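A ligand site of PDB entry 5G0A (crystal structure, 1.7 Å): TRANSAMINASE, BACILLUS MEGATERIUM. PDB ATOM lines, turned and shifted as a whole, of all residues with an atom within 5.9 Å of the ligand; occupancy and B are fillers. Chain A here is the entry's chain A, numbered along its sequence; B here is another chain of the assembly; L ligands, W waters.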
ATOM      1  N   LEU A  59     -24.330  13.617  -7.708  1.00  0.00           N
ATOM      2  CA  LEU A  59     -23.105  13.091  -8.348  1.00  0.00           C
ATOM      3  C   LEU A  59     -23.376  11.658  -8.815  1.00  0.00           C
ATOM      4  O   LEU A  59     -22.579  10.748  -8.602  1.00  0.00           O
ATOM      5  CB  LEU A  59     -21.900  13.155  -7.393  1.00  0.00           C
ATOM      6  CG  LEU A  59     -21.515  14.551  -6.885  1.00  0.00           C
ATOM      7  CD1 LEU A  59     -20.553  14.422  -5.697  1.00  0.00           C
ATOM      8  CD2 LEU A  59     -20.896  15.364  -8.018  1.00  0.00           C
ATOM      9  N   SER A 119     -16.180   4.090   4.388  1.00  0.00           N
ATOM     10  CA  SER A 119     -17.178   5.163   4.438  1.00  0.00           C
ATOM     11  C   SER A 119     -17.368   5.911   3.119  1.00  0.00           C
ATOM     12  O   SER A 119     -18.350   6.610   2.959  1.00  0.00           O
ATOM     13  CB  SER A 119     -16.862   6.162   5.559  1.00  0.00           C
ATOM     14  OG  SER A 119     -16.947   5.545   6.820  1.00  0.00           O
ATOM     15  N   THR A 120     -16.413   5.756   2.201  1.00  0.00           N
ATOM     16  CA  THR A 120     -16.488   6.476   0.921  1.00  0.00           C
ATOM     17  C   THR A 120     -15.973   5.648  -0.262  1.00  0.00           C
ATOM     18  O   THR A 120     -15.315   4.639  -0.064  1.00  0.00           O
ATOM     19  CB  THR A 120     -15.677   7.796   0.975  1.00  0.00           C
ATOM     20  OG1 THR A 120     -14.266   7.489   0.984  1.00  0.00           O
ATOM     21  CG2 THR A 120     -16.059   8.637   2.205  1.00  0.00           C
ATOM     22  N   GLY A 121     -16.285   6.100  -1.481  1.00  0.00           N
ATOM     23  CA  GLY A 121     -15.816   5.411  -2.694  1.00  0.00           C
ATOM     24  C   GLY A 121     -14.302   5.470  -2.789  1.00  0.00           C
ATOM     25  O   GLY A 121     -13.659   4.478  -3.186  1.00  0.00           O
ATOM     26  N   SER A 122     -13.711   6.617  -2.427  1.00  0.00           N
ATOM     27  CA  SER A 122     -12.237   6.764  -2.481  1.00  0.00           C
ATOM     28  C   SER A 122     -11.613   5.794  -1.511  1.00  0.00           C
ATOM     29  O   SER A 122     -10.608   5.127  -1.836  1.00  0.00           O
ATOM     30  CB  SER A 122     -11.795   8.205  -2.143  1.00  0.00           C
ATOM     31  OG  SER A 122     -12.175   9.065  -3.199  1.00  0.00           O
ATOM     32  N   GLU A 123     -12.197   5.665  -0.316  1.00  0.00           N
ATOM     33  CA  GLU A 123     -11.692   4.707   0.638  1.00  0.00           C
ATOM     34  C   GLU A 123     -11.824   3.269   0.097  1.00  0.00           C
ATOM     35  O   GLU A 123     -10.955   2.425   0.358  1.00  0.00           O
ATOM     36  CB  GLU A 123     -12.387   4.838   2.008  1.00  0.00           C
ATOM     37  CG  GLU A 123     -11.911   6.070   2.808  1.00  0.00           C
ATOM     38  CD  GLU A 123     -12.348   6.046   4.268  1.00  0.00           C
ATOM     39  OE1 GLU A 123     -13.300   5.291   4.618  1.00  0.00           O
ATOM     40  OE2 GLU A 123     -11.758   6.801   5.070  1.00  0.00           O
ATOM     41  N   VAL A 125     -11.619   2.372  -3.065  1.00  0.00           N
ATOM     42  CA  VAL A 125     -10.553   2.233  -4.065  1.00  0.00           C
ATOM     43  C   VAL A 125      -9.199   2.014  -3.367  1.00  0.00           C
ATOM     44  O   VAL A 125      -8.423   1.160  -3.766  1.00  0.00           O
ATOM     45  CB  VAL A 125     -10.567   3.434  -5.072  1.00  0.00           C
ATOM     46  CG1 VAL A 125      -9.328   3.406  -5.978  1.00  0.00           C
ATOM     47  CG2 VAL A 125     -11.801   3.332  -5.944  1.00  0.00           C
ATOM     48  N   TYR A 148     -11.529   8.278 -13.487  1.00  0.00           N
ATOM     49  CA  TYR A 148     -11.681   8.922 -12.178  1.00  0.00           C
ATOM     50  C   TYR A 148     -11.950   7.823 -11.144  1.00  0.00           C
ATOM     51  O   TYR A 148     -12.918   7.070 -11.284  1.00  0.00           O
ATOM     52  CB  TYR A 148     -12.815   9.954 -12.161  1.00  0.00           C
ATOM     53  CG  TYR A 148     -12.868  10.624 -10.793  1.00  0.00           C
ATOM     54  CD1 TYR A 148     -11.944  11.619 -10.451  1.00  0.00           C
ATOM     55  CD2 TYR A 148     -13.792  10.220  -9.818  1.00  0.00           C
ATOM     56  CE1 TYR A 148     -11.943  12.191  -9.191  1.00  0.00           C
ATOM     57  CE2 TYR A 148     -13.812  10.813  -8.555  1.00  0.00           C
ATOM     58  CZ  TYR A 148     -12.870  11.793  -8.247  1.00  0.00           C
ATOM     59  OH  TYR A 148     -12.875  12.393  -7.004  1.00  0.00           O
ATOM     60  N   HIS A 149     -11.069   7.708 -10.151  1.00  0.00           N
ATOM     61  CA  HIS A 149     -11.228   6.642  -9.150  1.00  0.00           C
ATOM     62  C   HIS A 149     -11.188   7.205  -7.735  1.00  0.00           C
ATOM     63  O   HIS A 149     -11.047   6.471  -6.759  1.00  0.00           O
ATOM     64  CB  HIS A 149     -10.140   5.558  -9.333  1.00  0.00           C
ATOM     65  CG  HIS A 149     -10.245   4.811 -10.631  1.00  0.00           C
ATOM     66  ND1 HIS A 149     -11.251   3.902 -10.880  1.00  0.00           N
ATOM     67  CD2 HIS A 149      -9.445   4.816 -11.731  1.00  0.00           C
ATOM     68  CE1 HIS A 149     -11.086   3.401 -12.105  1.00  0.00           C
ATOM     69  NE2 HIS A 149      -9.994   3.935 -12.629  1.00  0.00           N
ATOM     70  N   GLY A 150     -11.357   8.525  -7.646  1.00  0.00           N
ATOM     71  CA  GLY A 150     -11.441   9.170  -6.322  1.00  0.00           C
ATOM     72  C   GLY A 150     -10.291  10.144  -6.082  1.00  0.00           C
ATOM     73  O   GLY A 150      -9.470  10.408  -6.998  1.00  0.00           O
ATOM     74  N   TRP A 151     -10.208  10.699  -4.864  1.00  0.00           N
ATOM     75  CA  TRP A 151      -9.358  11.878  -4.658  1.00  0.00           C
ATOM     76  C   TRP A 151      -8.276  11.707  -3.602  1.00  0.00           C
ATOM     77  O   TRP A 151      -7.348  12.525  -3.512  1.00  0.00           O
ATOM     78  CB  TRP A 151     -10.260  13.094  -4.298  1.00  0.00           C
ATOM     79  CG  TRP A 151     -10.927  12.907  -2.957  1.00  0.00           C
ATOM     80  CD1 TRP A 151     -12.121  12.264  -2.718  1.00  0.00           C
ATOM     81  CD2 TRP A 151     -10.417  13.308  -1.676  1.00  0.00           C
ATOM     82  NE1 TRP A 151     -12.381  12.260  -1.368  1.00  0.00           N
ATOM     83  CE2 TRP A 151     -11.360  12.892  -0.712  1.00  0.00           C
ATOM     84  CE3 TRP A 151      -9.263  13.974  -1.256  1.00  0.00           C
ATOM     85  CZ2 TRP A 151     -11.206  13.153   0.657  1.00  0.00           C
ATOM     86  CZ3 TRP A 151      -9.089  14.214   0.111  1.00  0.00           C
ATOM     87  CH2 TRP A 151     -10.056  13.786   1.050  1.00  0.00           C
ATOM     88  N   GLU A 237     -13.218   1.676 -15.320  1.00  0.00           N
ATOM     89  CA  GLU A 237     -14.636   1.989 -15.156  1.00  0.00           C
ATOM     90  C   GLU A 237     -15.254   1.487 -16.456  1.00  0.00           C
ATOM     91  O   GLU A 237     -14.709   1.767 -17.516  1.00  0.00           O
ATOM     92  CB  GLU A 237     -14.871   3.498 -15.098  1.00  0.00           C
ATOM     93  CG  GLU A 237     -14.248   4.254 -13.927  1.00  0.00           C
ATOM     94  CD  GLU A 237     -14.374   5.764 -14.135  1.00  0.00           C
ATOM     95  OE1 GLU A 237     -15.445   6.339 -13.831  1.00  0.00           O
ATOM     96  OE2 GLU A 237     -13.406   6.362 -14.655  1.00  0.00           O
ATOM     97  N   GLY A 241     -17.053   7.711 -15.704  1.00  0.00           N
ATOM     98  CA  GLY A 241     -18.137   8.487 -15.061  1.00  0.00           C
ATOM     99  C   GLY A 241     -17.844   9.966 -15.267  1.00  0.00           C
ATOM    100  O   GLY A 241     -18.391  10.610 -16.162  1.00  0.00           O
ATOM    101  N   ALA A 242     -16.972  10.506 -14.434  1.00  0.00           N
ATOM    102  CA  ALA A 242     -16.590  11.920 -14.580  1.00  0.00           C
ATOM    103  C   ALA A 242     -15.961  12.166 -15.938  1.00  0.00           C
ATOM    104  O   ALA A 242     -16.263  13.182 -16.597  1.00  0.00           O
ATOM    105  CB  ALA A 242     -15.617  12.307 -13.455  1.00  0.00           C
ATOM    106  N   ASP A 269     -14.084  -0.628 -11.064  1.00  0.00           N
ATOM    107  CA  ASP A 269     -14.572   0.373 -10.149  1.00  0.00           C
ATOM    108  C   ASP A 269     -16.036   0.592 -10.436  1.00  0.00           C
ATOM    109  O   ASP A 269     -16.380   1.152 -11.461  1.00  0.00           O
ATOM    110  CB  ASP A 269     -13.767   1.677 -10.353  1.00  0.00           C
ATOM    111  CG  ASP A 269     -14.096   2.730  -9.328  1.00  0.00           C
ATOM    112  OD1 ASP A 269     -15.112   2.596  -8.598  1.00  0.00           O
ATOM    113  OD2 ASP A 269     -13.316   3.705  -9.221  1.00  0.00           O
ATOM    114  N   GLU A 270     -16.900   0.093  -9.547  1.00  0.00           N
ATOM    115  CA  GLU A 270     -18.357   0.223  -9.674  1.00  0.00           C
ATOM    116  C   GLU A 270     -18.922   1.364  -8.786  1.00  0.00           C
ATOM    117  O   GLU A 270     -20.119   1.428  -8.548  1.00  0.00           O
ATOM    118  CB  GLU A 270     -19.034  -1.104  -9.253  1.00  0.00           C
ATOM    119  CG  GLU A 270     -18.802  -2.242 -10.255  1.00  0.00           C
ATOM    120  CD  GLU A 270     -19.675  -2.127 -11.526  1.00  0.00           C
ATOM    121  OE1 GLU A 270     -20.644  -1.318 -11.555  1.00  0.00           O
ATOM    122  OE2 GLU A 270     -19.400  -2.847 -12.497  1.00  0.00           O
ATOM    123  N   VAL A 271     -18.084   2.286  -8.327  1.00  0.00           N
ATOM    124  CA  VAL A 271     -18.619   3.282  -7.390  1.00  0.00           C
ATOM    125  C   VAL A 271     -19.761   4.057  -8.041  1.00  0.00           C
ATOM    126  O   VAL A 271     -20.780   4.335  -7.403  1.00  0.00           O
ATOM    127  CB  VAL A 271     -17.499   4.203  -6.819  1.00  0.00           C
ATOM    128  CG1 VAL A 271     -18.095   5.415  -6.072  1.00  0.00           C
ATOM    129  CG2 VAL A 271     -16.588   3.407  -5.853  1.00  0.00           C
ATOM    130  N   LEU A 272     -19.601   4.429  -9.312  1.00  0.00           N
ATOM    131  CA  LEU A 272     -20.624   5.196  -9.998  1.00  0.00           C
ATOM    132  C   LEU A 272     -21.592   4.265 -10.752  1.00  0.00           C
ATOM    133  O   LEU A 272     -22.803   4.510 -10.740  1.00  0.00           O
ATOM    134  CB  LEU A 272     -19.985   6.238 -10.943  1.00  0.00           C
ATOM    135  CG  LEU A 272     -20.954   7.285 -11.503  1.00  0.00           C
ATOM    136  CD1 LEU A 272     -20.253   8.647 -11.604  1.00  0.00           C
ATOM    137  CD2 LEU A 272     -21.456   6.822 -12.867  1.00  0.00           C
ATOM    138  N   THR A 295     -15.108  -2.069  -6.515  1.00  0.00           N
ATOM    139  CA  THR A 295     -15.256  -1.035  -5.521  1.00  0.00           C
ATOM    140  C   THR A 295     -16.649  -0.408  -5.625  1.00  0.00           C
ATOM    141  O   THR A 295     -17.236  -0.293  -6.699  1.00  0.00           O
ATOM    142  CB  THR A 295     -14.156   0.037  -5.668  1.00  0.00           C
ATOM    143  OG1 THR A 295     -14.151   0.501  -7.028  1.00  0.00           O
ATOM    144  CG2 THR A 295     -12.803  -0.573  -5.379  1.00  0.00           C
ATOM    145  N   GLY A 297     -19.671   2.561  -3.822  1.00  0.00           N
ATOM    146  CA  GLY A 297     -19.997   3.771  -3.047  1.00  0.00           C
ATOM    147  C   GLY A 297     -21.291   4.294  -3.652  1.00  0.00           C
ATOM    148  O   GLY A 297     -22.035   3.509  -4.266  1.00  0.00           O
ATOM    149  N   LYS A 298     -21.566   5.585  -3.499  1.00  0.00           N
ATOM    150  CA  LYS A 298     -22.727   6.239  -4.156  1.00  0.00           C
ATOM    151  C   LYS A 298     -24.033   5.454  -4.013  1.00  0.00           C
ATOM    152  O   LYS A 298     -24.677   5.507  -2.971  1.00  0.00           O
ATOM    153  CB  LYS A 298     -22.354   6.549  -5.609  1.00  0.00           C
ATOM    154  CG  LYS A 298     -21.237   7.628  -5.640  1.00  0.00           C
ATOM    155  CD  LYS A 298     -20.919   8.113  -7.080  1.00  0.00           C
ATOM    156  CE  LYS A 298     -19.902   9.302  -7.128  1.00  0.00           C
ATOM    157  NZ  LYS A 298     -18.618   8.924  -7.714  1.00  0.00           N
ATOM    158  N   GLU B 123      -9.421  10.958   5.666  1.00  0.00           N
ATOM    159  CA  GLU B 123      -9.745  11.952   4.633  1.00  0.00           C
ATOM    160  C   GLU B 123      -9.374  13.377   5.062  1.00  0.00           C
ATOM    161  O   GLU B 123      -8.926  14.179   4.245  1.00  0.00           O
ATOM    162  CB  GLU B 123     -11.212  11.881   4.223  1.00  0.00           C
ATOM    163  CG  GLU B 123     -11.501  10.668   3.316  1.00  0.00           C
ATOM    164  CD  GLU B 123     -12.897  10.690   2.721  1.00  0.00           C
ATOM    165  OE1 GLU B 123     -13.755  11.460   3.218  1.00  0.00           O
ATOM    166  OE2 GLU B 123     -13.119   9.969   1.725  1.00  0.00           O
ATOM    167  N   VAL B 328     -13.163  17.110  -5.352  1.00  0.00           N
ATOM    168  CA  VAL B 328     -14.511  16.713  -4.975  1.00  0.00           C
ATOM    169  C   VAL B 328     -14.474  15.396  -4.215  1.00  0.00           C
ATOM    170  O   VAL B 328     -13.675  14.492  -4.529  1.00  0.00           O
ATOM    171  CB  VAL B 328     -15.463  16.634  -6.203  1.00  0.00           C
ATOM    172  CG1 VAL B 328     -14.924  15.673  -7.258  1.00  0.00           C
ATOM    173  CG2 VAL B 328     -16.901  16.275  -5.789  1.00  0.00           C
ATOM    174  N   SER B 329     -15.317  15.309  -3.196  1.00  0.00           N
ATOM    175  CA  SER B 329     -15.529  14.091  -2.421  1.00  0.00           C
ATOM    176  C   SER B 329     -17.049  13.965  -2.297  1.00  0.00           C
ATOM    177  O   SER B 329     -17.708  14.888  -1.821  1.00  0.00           O
ATOM    178  CB  SER B 329     -14.867  14.219  -1.036  1.00  0.00           C
ATOM    179  OG  SER B 329     -15.402  13.268  -0.144  1.00  0.00           O
ATOM    180  N   THR B 330     -17.623  12.836  -2.741  1.00  0.00           N
ATOM    181  CA  THR B 330     -19.098  12.737  -2.777  1.00  0.00           C
ATOM    182  C   THR B 330     -19.737  13.156  -1.437  1.00  0.00           C
ATOM    183  O   THR B 330     -20.595  14.060  -1.414  1.00  0.00           O
ATOM    184  CB  THR B 330     -19.567  11.309  -3.175  1.00  0.00           C
ATOM    185  OG1 THR B 330     -18.975  10.962  -4.443  1.00  0.00           O
ATOM    186  CG2 THR B 330     -21.088  11.265  -3.332  1.00  0.00           C
ATOM    187  N   TYR B 331     -19.334  12.512  -0.345  1.00  0.00           N
ATOM    188  CA  TYR B 331     -20.009  12.690   0.930  1.00  0.00           C
ATOM    189  C   TYR B 331     -19.473  13.848   1.785  1.00  0.00           C
ATOM    190  O   TYR B 331     -19.947  14.087   2.887  1.00  0.00           O
ATOM    191  CB  TYR B 331     -20.072  11.390   1.728  1.00  0.00           C
ATOM    192  CG  TYR B 331     -20.843  10.321   0.964  1.00  0.00           C
ATOM    193  CD1 TYR B 331     -22.017  10.658   0.278  1.00  0.00           C
ATOM    194  CD2 TYR B 331     -20.382   9.016   0.894  1.00  0.00           C
ATOM    195  CE1 TYR B 331     -22.725   9.695  -0.447  1.00  0.00           C
ATOM    196  CE2 TYR B 331     -21.103   8.044   0.178  1.00  0.00           C
ATOM    197  CZ  TYR B 331     -22.270   8.414  -0.491  1.00  0.00           C
ATOM    198  OH  TYR B 331     -23.018   7.491  -1.220  1.00  0.00           O
HETATM  199  N1  LIG L   1     -14.639   5.993  -8.355  1.00  0.00           N
HETATM  200  C1  LIG L   1     -15.556   6.407  -9.235  1.00  0.00           C
HETATM  201  C2  LIG L   1     -15.721   5.755 -10.590  1.00  0.00           C
HETATM  202  C3  LIG L   1     -16.471   7.494  -8.859  1.00  0.00           C
HETATM  203  O1  LIG L   1     -17.410   7.910  -9.733  1.00  0.00           O
HETATM  204  C4  LIG L   1     -16.345   8.086  -7.513  1.00  0.00           C
HETATM  205  C5  LIG L   1     -17.317   9.164  -7.065  1.00  0.00           C
HETATM  206  C6  LIG L   1     -15.281   7.555  -6.646  1.00  0.00           C
HETATM  207  C7  LIG L   1     -14.459   6.538  -7.115  1.00  0.00           C
HETATM  208  C8  LIG L   1     -14.966   8.125  -5.277  1.00  0.00           C
HETATM  209  O2  LIG L   1     -16.055   8.146  -4.399  1.00  0.00           O
HETATM  210  P1  LIG L   1     -16.092   9.214  -3.210  1.00  0.00           P
HETATM  211  O3  LIG L   1     -14.779   9.185  -2.467  1.00  0.00           O
HETATM  212  O4  LIG L   1     -16.403  10.541  -3.886  1.00  0.00           O
HETATM  213  O5  LIG L   1     -17.214   8.727  -2.358  1.00  0.00           O
HETATM  214  O   HOH W   1     -14.567  10.769  -0.308  1.00  0.00           O
HETATM  215  O   HOH W   2     -17.512  10.347  -0.253  1.00  0.00           O
HETATM  216  O   HOH W   3     -14.693  11.823  -5.442  1.00  0.00           O
HETATM  217  O   HOH W   4     -16.132   8.596 -12.359  1.00  0.00           O
HETATM  218  O   HOH W   5     -19.671   7.522  -2.609  1.00  0.00           O
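Thr 120 touches the ligand. Tyr 148 touches the ligand (O to C2, 3.2 Å). His 149 touches the ligand (C to C7, 3.4 Å). Gly 150 touches the ligand (N to C7, 3.7 Å). Glu 237 touches the ligand (OE1 to C2, 3.3 Å). CG1 of Val 271 touches C4 of the ligand (3.5 Å). Leu 272 touches the ligand (CB to O1, 3.3 Å). C of Ser 329 of chain B touches O4 of the ligand (3.8 Å). Hydrophobic or aromatic side chains that line the ligand: Tyr 148, Val 271 and Leu 272. Within 4 Å of the ligand: Thr 120, Gly 121, Ser 122, Tyr 148, His 149, Gly 150, Glu 237, Asp 269, Val 271, Leu 272, Lys 298, Ser 329 of chain B and Thr 330 of chain B. The nearest printed residue that does not touch the ligand is Trp 151 (4.1 Å).
Water W3 lies within hydrogen-bond range of the side-chain hydroxyl (OH) of Tyr 148 (2.5 Å), an oxygen (O4) of the ligand (2.6 Å) and the backbone carbonyl oxygen (O) of Val 328 of chain B (3.0 Å). Water W2 lies within hydrogen-bond range of O5 of the ligand (2.7 Å) and N of Tyr 331 of chain B (2.8 Å). Water W1 lies within hydrogen-bond range of the side-chain carboxylate of Glu 123 of chain B (2.6 Å), the side-chain hydroxyl of Ser 329 of chain B (2.6 Å), an oxygen (O3) of the ligand (2.7 Å) and the indole nitrogen of Trp 151 (2.9 Å). Water W5 lies within hydrogen-bond range of an oxygen (O5) of the ligand and the backbone NH (N) of Lys 298. Water W4 lies within hydrogen-bond range of OE1 of Glu 237, N of Ala 242 and O1 of the ligand.
The side-chain hydroxyl (OH) of Tyr 331 of chain B is in hydrogen-bond range of the backbone carbonyl oxygen (O) of Lys 298, 3.1 Å away. OG of Ser 122 lies within hydrogen-bond range of N of Trp 151, at 3.1 Å. The backbone NH (N) of Tyr 148 sits at hydrogen-bond distance from the side-chain carboxylate (OE2) of Glu 237, at 2.9 Å. O of Val 328 of chain B lies within hydrogen-bond range of OH of Tyr 148, 3.3 Å away. The side-chain carboxylate of Glu 237 is in hydrogen-bond range of the backbone NH of Gly 241, 2.8 Å away. The side-chain hydroxyl (OG1) of Thr 120 is in hydrogen-bond range of the side-chain carboxylate (OE2) of Glu 123 of chain B (2.8 Å). OG1 of Thr 120 lies within hydrogen-bond range of N of Glu 123 of chain A. OG of Ser 329 of chain B sits close to NE1 of Trp 151, at 3.4 Å.
The side-chain amino group (NZ) of Lys 298 is covalently linked to a carbon (C5) of the ligand. N of Thr 330 of chain B sits at hydrogen-bond distance from O4 of the ligand (2.8 Å). O4 of the ligand is in hydrogen-bond range of OG1 of Thr 330 of chain B (2.7 Å). N of Ser 122 sits at hydrogen-bond distance from O3 of the ligand, at 2.8 Å. O3 of the ligand is in hydrogen-bond range of OG of Ser 122 (2.7 Å). The side-chain carboxylate (OD2) of Asp 269 lies within hydrogen-bond range of a nitrogen (N1) of the ligand (2.8 Å). An oxygen (O5) of the ligand lies within hydrogen-bond range of the backbone NH of Gly 121 (2.9 Å).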
